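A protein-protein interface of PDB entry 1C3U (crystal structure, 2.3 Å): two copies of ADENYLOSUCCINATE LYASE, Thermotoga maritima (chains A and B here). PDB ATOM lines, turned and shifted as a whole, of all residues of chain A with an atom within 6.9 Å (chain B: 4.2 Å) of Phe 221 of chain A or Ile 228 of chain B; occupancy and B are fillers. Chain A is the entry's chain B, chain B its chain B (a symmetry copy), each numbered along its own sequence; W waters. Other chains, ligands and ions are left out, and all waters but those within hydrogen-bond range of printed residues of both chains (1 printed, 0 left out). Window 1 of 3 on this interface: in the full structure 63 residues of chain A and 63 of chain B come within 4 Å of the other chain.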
ATOM      1  N   ARG A 167      -7.311 -26.656   2.496  1.00  0.00           N
ATOM      2  CA  ARG A 167      -6.408 -27.043   1.428  1.00  0.00           C
ATOM      3  C   ARG A 167      -6.490 -26.137   0.198  1.00  0.00           C
ATOM      4  O   ARG A 167      -5.482 -25.708  -0.401  1.00  0.00           O
ATOM      5  CB  ARG A 167      -6.659 -28.517   1.040  1.00  0.00           C
ATOM      6  CG  ARG A 167      -6.110 -29.528   2.078  1.00  0.00           C
ATOM      7  CD  ARG A 167      -6.791 -30.881   1.779  1.00  0.00           C
ATOM      8  NE  ARG A 167      -6.545 -31.894   2.825  1.00  0.00           N
ATOM      9  CZ  ARG A 167      -7.275 -32.989   2.994  1.00  0.00           C
ATOM     10  NH1 ARG A 167      -8.332 -33.290   2.213  1.00  0.00           N
ATOM     11  NH2 ARG A 167      -6.980 -33.896   3.920  1.00  0.00           N
ATOM     12  N   ARG A 170      -4.730 -22.874   0.810  1.00  0.00           N
ATOM     13  CA  ARG A 170      -3.316 -22.959   0.647  1.00  0.00           C
ATOM     14  C   ARG A 170      -2.949 -23.072  -0.820  1.00  0.00           C
ATOM     15  O   ARG A 170      -1.984 -22.400  -1.231  1.00  0.00           O
ATOM     16  CB  ARG A 170      -2.595 -24.132   1.423  1.00  0.00           C
ATOM     17  CG  ARG A 170      -2.730 -23.785   2.915  1.00  0.00           C
ATOM     18  CD  ARG A 170      -2.398 -24.900   3.887  1.00  0.00           C
ATOM     19  NE  ARG A 170      -2.891 -26.195   3.447  1.00  0.00           N
ATOM     20  CZ  ARG A 170      -2.624 -27.036   2.474  1.00  0.00           C
ATOM     21  NH1 ARG A 170      -1.689 -26.827   1.577  1.00  0.00           N
ATOM     22  NH2 ARG A 170      -3.207 -28.175   2.233  1.00  0.00           N
ATOM     23  N   ALA A 171      -3.718 -23.860  -1.574  1.00  0.00           N
ATOM     24  CA  ALA A 171      -3.473 -23.886  -3.008  1.00  0.00           C
ATOM     25  C   ALA A 171      -3.649 -22.498  -3.661  1.00  0.00           C
ATOM     26  O   ALA A 171      -2.848 -22.172  -4.546  1.00  0.00           O
ATOM     27  CB  ALA A 171      -4.344 -24.921  -3.726  1.00  0.00           C
ATOM     28  N   ILE A 172      -4.597 -21.671  -3.273  1.00  0.00           N
ATOM     29  CA  ILE A 172      -4.713 -20.295  -3.773  1.00  0.00           C
ATOM     30  C   ILE A 172      -3.453 -19.508  -3.403  1.00  0.00           C
ATOM     31  O   ILE A 172      -2.870 -18.821  -4.272  1.00  0.00           O
ATOM     32  CB  ILE A 172      -5.979 -19.581  -3.230  1.00  0.00           C
ATOM     33  CG1 ILE A 172      -7.236 -20.218  -3.855  1.00  0.00           C
ATOM     34  CG2 ILE A 172      -5.975 -18.079  -3.439  1.00  0.00           C
ATOM     35  CD1 ILE A 172      -8.536 -20.086  -3.030  1.00  0.00           C
ATOM     36  N   GLU A 174      -0.502 -20.756  -2.911  1.00  0.00           N
ATOM     37  CA  GLU A 174       0.638 -21.235  -3.704  1.00  0.00           C
ATOM     38  C   GLU A 174       0.738 -20.626  -5.101  1.00  0.00           C
ATOM     39  O   GLU A 174       1.825 -20.369  -5.655  1.00  0.00           O
ATOM     40  CB  GLU A 174       0.586 -22.772  -3.818  1.00  0.00           C
ATOM     41  CG  GLU A 174       0.944 -23.389  -2.461  1.00  0.00           C
ATOM     42  CD  GLU A 174       2.331 -24.013  -2.528  1.00  0.00           C
ATOM     43  OE1 GLU A 174       2.973 -23.915  -3.593  1.00  0.00           O
ATOM     44  OE2 GLU A 174       2.775 -24.637  -1.546  1.00  0.00           O
ATOM     45  N   VAL A 175      -0.397 -20.279  -5.661  1.00  0.00           N
ATOM     46  CA  VAL A 175      -0.458 -19.838  -7.051  1.00  0.00           C
ATOM     47  C   VAL A 175      -0.540 -18.332  -7.167  1.00  0.00           C
ATOM     48  O   VAL A 175      -0.597 -17.783  -8.264  1.00  0.00           O
ATOM     49  CB  VAL A 175      -1.626 -20.711  -7.552  1.00  0.00           C
ATOM     50  CG1 VAL A 175      -2.972 -20.052  -7.647  1.00  0.00           C
ATOM     51  CG2 VAL A 175      -1.177 -21.584  -8.693  1.00  0.00           C
ATOM     52  N   ARG A 216       7.029 -24.530 -11.837  1.00  0.00           N
ATOM     53  CA  ARG A 216       5.776 -25.264 -12.048  1.00  0.00           C
ATOM     54  C   ARG A 216       5.372 -26.164 -10.897  1.00  0.00           C
ATOM     55  O   ARG A 216       4.305 -26.793 -10.894  1.00  0.00           O
ATOM     56  CB  ARG A 216       5.831 -26.079 -13.358  1.00  0.00           C
ATOM     57  CG  ARG A 216       4.966 -25.465 -14.476  1.00  0.00           C
ATOM     58  CD  ARG A 216       5.233 -24.012 -14.726  1.00  0.00           C
ATOM     59  NE  ARG A 216       4.228 -23.373 -15.562  1.00  0.00           N
ATOM     60  CZ  ARG A 216       4.278 -22.113 -16.031  1.00  0.00           C
ATOM     61  NH1 ARG A 216       3.288 -21.620 -16.787  1.00  0.00           N
ATOM     62  NH2 ARG A 216       5.295 -21.377 -15.660  1.00  0.00           N
ATOM     63  N   ASP A 217       6.181 -26.242  -9.834  1.00  0.00           N
ATOM     64  CA  ASP A 217       5.748 -26.964  -8.637  1.00  0.00           C
ATOM     65  C   ASP A 217       4.534 -26.316  -7.973  1.00  0.00           C
ATOM     66  O   ASP A 217       3.760 -27.053  -7.317  1.00  0.00           O
ATOM     67  CB  ASP A 217       6.888 -27.120  -7.626  1.00  0.00           C
ATOM     68  CG  ASP A 217       7.445 -25.802  -7.112  1.00  0.00           C
ATOM     69  OD1 ASP A 217       7.430 -25.492  -5.893  1.00  0.00           O
ATOM     70  OD2 ASP A 217       7.942 -25.034  -7.971  1.00  0.00           O
ATOM     71  N   ARG A 218       4.307 -25.018  -8.105  1.00  0.00           N
ATOM     72  CA  ARG A 218       3.167 -24.335  -7.522  1.00  0.00           C
ATOM     73  C   ARG A 218       1.901 -24.820  -8.223  1.00  0.00           C
ATOM     74  O   ARG A 218       0.860 -25.138  -7.599  1.00  0.00           O
ATOM     75  CB  ARG A 218       3.213 -22.794  -7.656  1.00  0.00           C
ATOM     76  CG  ARG A 218       4.500 -22.141  -7.101  1.00  0.00           C
ATOM     77  CD  ARG A 218       4.450 -20.617  -7.329  1.00  0.00           C
ATOM     78  NE  ARG A 218       5.540 -19.928  -6.696  1.00  0.00           N
ATOM     79  CZ  ARG A 218       5.700 -19.803  -5.376  1.00  0.00           C
ATOM     80  NH1 ARG A 218       4.796 -20.271  -4.528  1.00  0.00           N
ATOM     81  NH2 ARG A 218       6.804 -19.225  -4.935  1.00  0.00           N
ATOM     82  N   HIS A 219       1.963 -24.871  -9.545  1.00  0.00           N
ATOM     83  CA  HIS A 219       0.773 -25.323 -10.304  1.00  0.00           C
ATOM     84  C   HIS A 219       0.432 -26.778 -10.013  1.00  0.00           C
ATOM     85  O   HIS A 219      -0.752 -27.149  -9.932  1.00  0.00           O
ATOM     86  CB  HIS A 219       1.014 -25.099 -11.793  1.00  0.00           C
ATOM     87  CG  HIS A 219       1.557 -23.743 -12.108  1.00  0.00           C
ATOM     88  ND1 HIS A 219       2.876 -23.415 -11.893  1.00  0.00           N
ATOM     89  CD2 HIS A 219       0.983 -22.618 -12.596  1.00  0.00           C
ATOM     90  CE1 HIS A 219       3.089 -22.150 -12.240  1.00  0.00           C
ATOM     91  NE2 HIS A 219       1.964 -21.659 -12.687  1.00  0.00           N
ATOM     92  N   ALA A 220       1.448 -27.630  -9.866  1.00  0.00           N
ATOM     93  CA  ALA A 220       1.252 -29.037  -9.556  1.00  0.00           C
ATOM     94  C   ALA A 220       0.644 -29.220  -8.152  1.00  0.00           C
ATOM     95  O   ALA A 220      -0.197 -30.104  -7.981  1.00  0.00           O
ATOM     96  CB  ALA A 220       2.514 -29.874  -9.587  1.00  0.00           C
ATOM     97  N   PHE A 221       1.027 -28.385  -7.219  1.00  0.00           N
ATOM     98  CA  PHE A 221       0.457 -28.367  -5.891  1.00  0.00           C
ATOM     99  C   PHE A 221      -1.025 -28.028  -5.932  1.00  0.00           C
ATOM    100  O   PHE A 221      -1.882 -28.622  -5.296  1.00  0.00           O
ATOM    101  CB  PHE A 221       1.226 -27.321  -5.004  1.00  0.00           C
ATOM    102  CG  PHE A 221       0.683 -27.398  -3.613  1.00  0.00           C
ATOM    103  CD1 PHE A 221       1.166 -28.311  -2.698  1.00  0.00           C
ATOM    104  CD2 PHE A 221      -0.403 -26.576  -3.256  1.00  0.00           C
ATOM    105  CE1 PHE A 221       0.640 -28.384  -1.418  1.00  0.00           C
ATOM    106  CE2 PHE A 221      -0.921 -26.659  -1.968  1.00  0.00           C
ATOM    107  CZ  PHE A 221      -0.422 -27.589  -1.058  1.00  0.00           C
ATOM    108  N   TYR A 222      -1.397 -27.021  -6.714  1.00  0.00           N
ATOM    109  CA  TYR A 222      -2.762 -26.549  -6.847  1.00  0.00           C
ATOM    110  C   TYR A 222      -3.599 -27.672  -7.424  1.00  0.00           C
ATOM    111  O   TYR A 222      -4.680 -27.982  -6.972  1.00  0.00           O
ATOM    112  CB  TYR A 222      -2.764 -25.397  -7.864  1.00  0.00           C
ATOM    113  CG  TYR A 222      -4.043 -24.727  -8.276  1.00  0.00           C
ATOM    114  CD1 TYR A 222      -4.435 -23.598  -7.555  1.00  0.00           C
ATOM    115  CD2 TYR A 222      -4.830 -25.141  -9.328  1.00  0.00           C
ATOM    116  CE1 TYR A 222      -5.582 -22.892  -7.902  1.00  0.00           C
ATOM    117  CE2 TYR A 222      -5.954 -24.441  -9.725  1.00  0.00           C
ATOM    118  CZ  TYR A 222      -6.317 -23.306  -8.980  1.00  0.00           C
ATOM    119  OH  TYR A 222      -7.451 -22.597  -9.315  1.00  0.00           O
ATOM    120  N   LEU A 223      -3.108 -28.255  -8.522  1.00  0.00           N
ATOM    121  CA  LEU A 223      -3.846 -29.260  -9.216  1.00  0.00           C
ATOM    122  C   LEU A 223      -3.912 -30.555  -8.404  1.00  0.00           C
ATOM    123  O   LEU A 223      -4.955 -31.248  -8.470  1.00  0.00           O
ATOM    124  CB  LEU A 223      -3.280 -29.539 -10.650  1.00  0.00           C
ATOM    125  CG  LEU A 223      -3.427 -28.305 -11.589  1.00  0.00           C
ATOM    126  CD1 LEU A 223      -2.437 -28.342 -12.767  1.00  0.00           C
ATOM    127  CD2 LEU A 223      -4.848 -28.150 -12.123  1.00  0.00           C
ATOM    128  N   SER A 224      -2.831 -30.937  -7.694  1.00  0.00           N
ATOM    129  CA  SER A 224      -2.960 -32.057  -6.745  1.00  0.00           C
ATOM    130  C   SER A 224      -4.037 -31.775  -5.710  1.00  0.00           C
ATOM    131  O   SER A 224      -4.785 -32.694  -5.498  1.00  0.00           O
ATOM    132  CB  SER A 224      -1.647 -32.138  -5.925  1.00  0.00           C
ATOM    133  OG  SER A 224      -0.655 -32.572  -6.878  1.00  0.00           O
ATOM    134  N   THR A 225      -4.099 -30.556  -5.140  1.00  0.00           N
ATOM    135  CA  THR A 225      -5.198 -30.227  -4.245  1.00  0.00           C
ATOM    136  C   THR A 225      -6.562 -30.363  -4.927  1.00  0.00           C
ATOM    137  O   THR A 225      -7.504 -30.904  -4.335  1.00  0.00           O
ATOM    138  CB  THR A 225      -5.090 -28.759  -3.763  1.00  0.00           C
ATOM    139  OG1 THR A 225      -3.885 -28.598  -3.006  1.00  0.00           O
ATOM    140  CG2 THR A 225      -6.302 -28.272  -2.991  1.00  0.00           C
ATOM    141  N   LEU A 226      -6.700 -29.893  -6.157  1.00  0.00           N
ATOM    142  CA  LEU A 226      -7.997 -30.052  -6.854  1.00  0.00           C
ATOM    143  C   LEU A 226      -8.381 -31.511  -6.990  1.00  0.00           C
ATOM    144  O   LEU A 226      -9.535 -31.892  -6.777  1.00  0.00           O
ATOM    145  CB  LEU A 226      -7.951 -29.375  -8.226  1.00  0.00           C
ATOM    146  CG  LEU A 226      -8.447 -27.912  -8.230  1.00  0.00           C
ATOM    147  CD1 LEU A 226      -8.021 -27.075  -7.069  1.00  0.00           C
ATOM    148  CD2 LEU A 226      -8.264 -27.259  -9.586  1.00  0.00           C
ATOM    149  N   SER A 291       0.783 -32.529 -14.630  1.00  0.00           N
ATOM    150  CA  SER A 291       1.266 -31.352 -13.888  1.00  0.00           C
ATOM    151  C   SER A 291       2.568 -31.603 -13.131  1.00  0.00           C
ATOM    152  O   SER A 291       3.358 -30.642 -13.061  1.00  0.00           O
ATOM    153  CB  SER A 291       0.225 -30.880 -12.848  1.00  0.00           C
ATOM    154  OG  SER A 291      -1.022 -30.943 -13.584  1.00  0.00           O
ATOM    155  N   LEU A 292       2.765 -32.756 -12.513  1.00  0.00           N
ATOM    156  CA  LEU A 292       4.005 -33.107 -11.844  1.00  0.00           C
ATOM    157  C   LEU A 292       5.184 -33.237 -12.808  1.00  0.00           C
ATOM    158  O   LEU A 292       6.245 -32.737 -12.382  1.00  0.00           O
ATOM    159  CB  LEU A 292       3.847 -34.417 -11.040  1.00  0.00           C
ATOM    160  CG  LEU A 292       2.915 -34.355  -9.809  1.00  0.00           C
ATOM    161  CD1 LEU A 292       2.461 -35.802  -9.536  1.00  0.00           C
ATOM    162  CD2 LEU A 292       3.580 -33.762  -8.594  1.00  0.00           C
ATOM    163  N   ILE A 295       7.069 -30.136 -13.920  1.00  0.00           N
ATOM    164  CA  ILE A 295       7.966 -29.474 -12.967  1.00  0.00           C
ATOM    165  C   ILE A 295       9.382 -29.444 -13.523  1.00  0.00           C
ATOM    166  O   ILE A 295       9.984 -28.355 -13.463  1.00  0.00           O
ATOM    167  CB  ILE A 295       7.920 -30.054 -11.547  1.00  0.00           C
ATOM    168  CG1 ILE A 295       6.519 -29.832 -10.956  1.00  0.00           C
ATOM    169  CG2 ILE A 295       9.003 -29.500 -10.628  1.00  0.00           C
ATOM    170  CD1 ILE A 295       6.249 -30.632  -9.699  1.00  0.00           C
ATOM    171  N   ASN B 164       9.059 -26.652  -0.199  1.00  0.00           N
ATOM    172  CA  ASN B 164       8.782 -28.032   0.185  1.00  0.00           C
ATOM    173  C   ASN B 164       8.947 -28.300   1.666  1.00  0.00           C
ATOM    174  O   ASN B 164       8.292 -29.231   2.150  1.00  0.00           O
ATOM    175  CB  ASN B 164       9.637 -29.013  -0.621  1.00  0.00           C
ATOM    176  CG  ASN B 164       9.209 -29.101  -2.054  1.00  0.00           C
ATOM    177  OD1 ASN B 164       8.010 -29.062  -2.328  1.00  0.00           O
ATOM    178  ND2 ASN B 164      10.089 -29.230  -3.038  1.00  0.00           N
ATOM    179  N   ARG B 167       5.548 -27.309   2.866  1.00  0.00           N
ATOM    180  CA  ARG B 167       4.617 -28.324   2.408  1.00  0.00           C
ATOM    181  C   ARG B 167       4.692 -29.627   3.205  1.00  0.00           C
ATOM    182  O   ARG B 167       3.680 -30.242   3.602  1.00  0.00           O
ATOM    183  CB  ARG B 167       4.834 -28.590   0.902  1.00  0.00           C
ATOM    184  CG  ARG B 167       4.288 -27.462  -0.008  1.00  0.00           C
ATOM    185  CD  ARG B 167       4.938 -27.657  -1.394  1.00  0.00           C
ATOM    186  NE  ARG B 167       4.695 -26.524  -2.310  1.00  0.00           N
ATOM    187  CZ  ARG B 167       5.407 -26.276  -3.401  1.00  0.00           C
ATOM    188  NH1 ARG B 167       6.444 -27.048  -3.788  1.00  0.00           N
ATOM    189  NH2 ARG B 167       5.115 -25.272  -4.221  1.00  0.00           N
ATOM    190  N   ARG B 170       3.002 -29.262   6.542  1.00  0.00           N
ATOM    191  CA  ARG B 170       1.584 -29.392   6.470  1.00  0.00           C
ATOM    192  C   ARG B 170       1.187 -30.838   6.242  1.00  0.00           C
ATOM    193  O   ARG B 170       0.226 -31.287   6.896  1.00  0.00           O
ATOM    194  CB  ARG B 170       0.857 -28.507   5.381  1.00  0.00           C
ATOM    195  CG  ARG B 170       1.027 -27.052   5.850  1.00  0.00           C
ATOM    196  CD  ARG B 170       0.694 -25.984   4.827  1.00  0.00           C
ATOM    197  NE  ARG B 170       1.155 -26.322   3.490  1.00  0.00           N
ATOM    198  CZ  ARG B 170       0.855 -27.215   2.576  1.00  0.00           C
ATOM    199  NH1 ARG B 170      -0.093 -28.110   2.727  1.00  0.00           N
ATOM    200  NH2 ARG B 170       1.413 -27.369   1.409  1.00  0.00           N
ATOM    201  N   SER B 224       0.795 -37.019  -2.170  1.00  0.00           N
ATOM    202  CA  SER B 224       0.922 -35.981  -3.208  1.00  0.00           C
ATOM    203  C   SER B 224       2.024 -34.993  -2.861  1.00  0.00           C
ATOM    204  O   SER B 224       2.759 -34.718  -3.773  1.00  0.00           O
ATOM    205  CB  SER B 224      -0.376 -35.134  -3.194  1.00  0.00           C
ATOM    206  OG  SER B 224      -1.394 -36.029  -3.688  1.00  0.00           O
ATOM    207  N   THR B 225       2.119 -34.530  -1.600  1.00  0.00           N
ATOM    208  CA  THR B 225       3.241 -33.685  -1.218  1.00  0.00           C
ATOM    209  C   THR B 225       4.588 -34.378  -1.437  1.00  0.00           C
ATOM    210  O   THR B 225       5.532 -33.759  -1.945  1.00  0.00           O
ATOM    211  CB  THR B 225       3.168 -33.327   0.287  1.00  0.00           C
ATOM    212  OG1 THR B 225       1.981 -32.565   0.534  1.00  0.00           O
ATOM    213  CG2 THR B 225       4.403 -32.620   0.814  1.00  0.00           C
ATOM    214  N   LEU B 226       4.711 -35.646  -1.076  1.00  0.00           N
ATOM    215  CA  LEU B 226       5.991 -36.350  -1.318  1.00  0.00           C
ATOM    216  C   LEU B 226       6.346 -36.368  -2.791  1.00  0.00           C
ATOM    217  O   LEU B 226       7.497 -36.145  -3.174  1.00  0.00           O
ATOM    218  CB  LEU B 226       5.931 -37.773  -0.758  1.00  0.00           C
ATOM    219  CG  LEU B 226       6.452 -37.908   0.690  1.00  0.00           C
ATOM    220  CD1 LEU B 226       6.063 -36.815   1.629  1.00  0.00           C
ATOM    221  CD2 LEU B 226       6.254 -39.312   1.229  1.00  0.00           C
ATOM    222  N   ALA B 227       5.352 -36.517  -3.675  1.00  0.00           N
ATOM    223  CA  ALA B 227       5.682 -36.623  -5.106  1.00  0.00           C
ATOM    224  C   ALA B 227       6.187 -35.267  -5.607  1.00  0.00           C
ATOM    225  O   ALA B 227       7.019 -35.243  -6.496  1.00  0.00           O
ATOM    226  CB  ALA B 227       4.478 -37.029  -5.934  1.00  0.00           C
ATOM    227  N   ILE B 228       5.631 -34.175  -5.068  1.00  0.00           N
ATOM    228  CA  ILE B 228       6.077 -32.847  -5.480  1.00  0.00           C
ATOM    229  C   ILE B 228       7.495 -32.548  -4.977  1.00  0.00           C
ATOM    230  O   ILE B 228       8.297 -31.999  -5.770  1.00  0.00           O
ATOM    231  CB  ILE B 228       5.080 -31.775  -5.002  1.00  0.00           C
ATOM    232  CG1 ILE B 228       3.731 -31.964  -5.752  1.00  0.00           C
ATOM    233  CG2 ILE B 228       5.633 -30.367  -5.147  1.00  0.00           C
ATOM    234  CD1 ILE B 228       2.647 -31.107  -5.033  1.00  0.00           C
ATOM    235  N   VAL B 229       7.834 -32.953  -3.738  1.00  0.00           N
ATOM    236  CA  VAL B 229       9.223 -32.822  -3.310  1.00  0.00           C
ATOM    237  C   VAL B 229      10.146 -33.552  -4.281  1.00  0.00           C
ATOM    238  O   VAL B 229      11.175 -33.027  -4.730  1.00  0.00           O
ATOM    239  CB  VAL B 229       9.481 -33.288  -1.873  1.00  0.00           C
ATOM    240  CG1 VAL B 229      10.940 -33.022  -1.466  1.00  0.00           C
ATOM    241  CG2 VAL B 229       8.526 -32.684  -0.857  1.00  0.00           C
ATOM    242  N   ALA B 230       9.799 -34.758  -4.699  1.00  0.00           N
ATOM    243  CA  ALA B 230      10.645 -35.581  -5.551  1.00  0.00           C
ATOM    244  C   ALA B 230      10.833 -34.954  -6.929  1.00  0.00           C
ATOM    245  O   ALA B 230      11.889 -35.093  -7.547  1.00  0.00           O
ATOM    246  CB  ALA B 230      10.015 -36.985  -5.710  1.00  0.00           C
ATOM    247  N   ALA B 231       9.827 -34.289  -7.456  1.00  0.00           N
ATOM    248  CA  ALA B 231       9.890 -33.674  -8.789  1.00  0.00           C
ATOM    249  C   ALA B 231      10.787 -32.453  -8.781  1.00  0.00           C
ATOM    250  O   ALA B 231      11.449 -32.196  -9.772  1.00  0.00           O
ATOM    251  CB  ALA B 231       8.515 -33.263  -9.334  1.00  0.00           C
ATOM    252  N   GLY B 232      10.905 -31.740  -7.668  1.00  0.00           N
ATOM    253  CA  GLY B 232      11.899 -30.688  -7.519  1.00  0.00           C
ATOM    254  C   GLY B 232      13.310 -31.286  -7.525  1.00  0.00           C
ATOM    255  O   GLY B 232      14.222 -30.660  -8.079  1.00  0.00           O
HETATM  256  O   HOH W   1       1.592 -25.056   0.759  1.00  0.00           O
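NH2 of Arg 167 of chain B is in salt-bridge range of OE1 of Glu 174 of chain A (2.6 Å). The guanidinium group (NH1) of Arg 170 of chain B lies close to the guanidinium group (NH1) of Arg 170 of chain A (2.3 Å). The side-chain carboxylate (OD1) of Asp 217 of chain A lies within salt-bridge range of the guanidinium group (NH1) of Arg 167 of chain B (2.8 Å).
Phe 221 of chain A touches just these residues of chain B: Arg 167, Arg 170 and Ile 228. Ile 228 of chain B touches just these residues of chain A: Phe 221 (3.6 Å) and Leu 292 (3.4 Å). Printed residues of chain B within 4 Å of Arg 218 of chain A: Arg 167 (3.9 Å). Of the printed residues of chain A, Ala 231 of chain B touches Leu 292 and Ile 295. Printed residues of chain B within 4 Å of Leu 292 of chain A: Ile 228 and Ala 231. Printed residues of chain B within 4 Å of Arg 170 of chain A: Arg 170. Of the printed residues of chain B, Asp 217 of chain A touches Arg 167 (2.8 Å). Asn 164 of chain B touches none of the printed residues of chain A. The nearest printed residue of chain B that does not touch Phe 221 of chain A is Thr 225 of chain B (4.8 Å). The nearest residue of chain A that does not touch Ile 228 of chain B is Ser 224 of chain A (4.1 Å).
Among the printed residues, pairs that only touch across the chains: Phe 221 of chain A with Arg 170 of chain B, Leu 292 of chain A with Ile 228 of chain B, Ile 295 of chain A with Ala 231 of chain B, Phe 221 of chain A with Ile 228 of chain B, Leu 292 of chain A with Ala 231 of chain B, Arg 218 of chain A with Arg 167 of chain B and Phe 221 of chain A with Arg 167 of chain B.
Arg 170 of chain B touches its own counterpart, Arg 170 of chain A. 5 positions are printed for both chains.
Water W1 bridges NH2 of Arg 170 of chain B (2.4 Å) and OE2 of Glu 174 of chain A (2.6 Å).
Among the printed residues, Asp or Glu carboxylates within 4 Å of a Lys or Arg side-chain nitrogen of the other chain: Glu 174 of chain A with Arg 167 of chain B (2.6 Å) and Asp 217 of chain A with Arg 167 of chain B (2.8 Å).
The side-chain amide oxygen (OD1) of Asn 164 of chain B lies within hydrogen-bond range of the guanidinium group (NH1) of Arg 167 of chain B, at 2.9 Å. The backbone carbonyl oxygen (O) of Glu 174 of chain A lies close to the guanidinium group (NH1) of Arg 218 of chain A, 3.2 Å away. The side-chain hydroxyl (OG1) of Thr 225 of chain A is in hydrogen-bond range of the backbone carbonyl oxygen (O) of Phe 221 of chain A.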
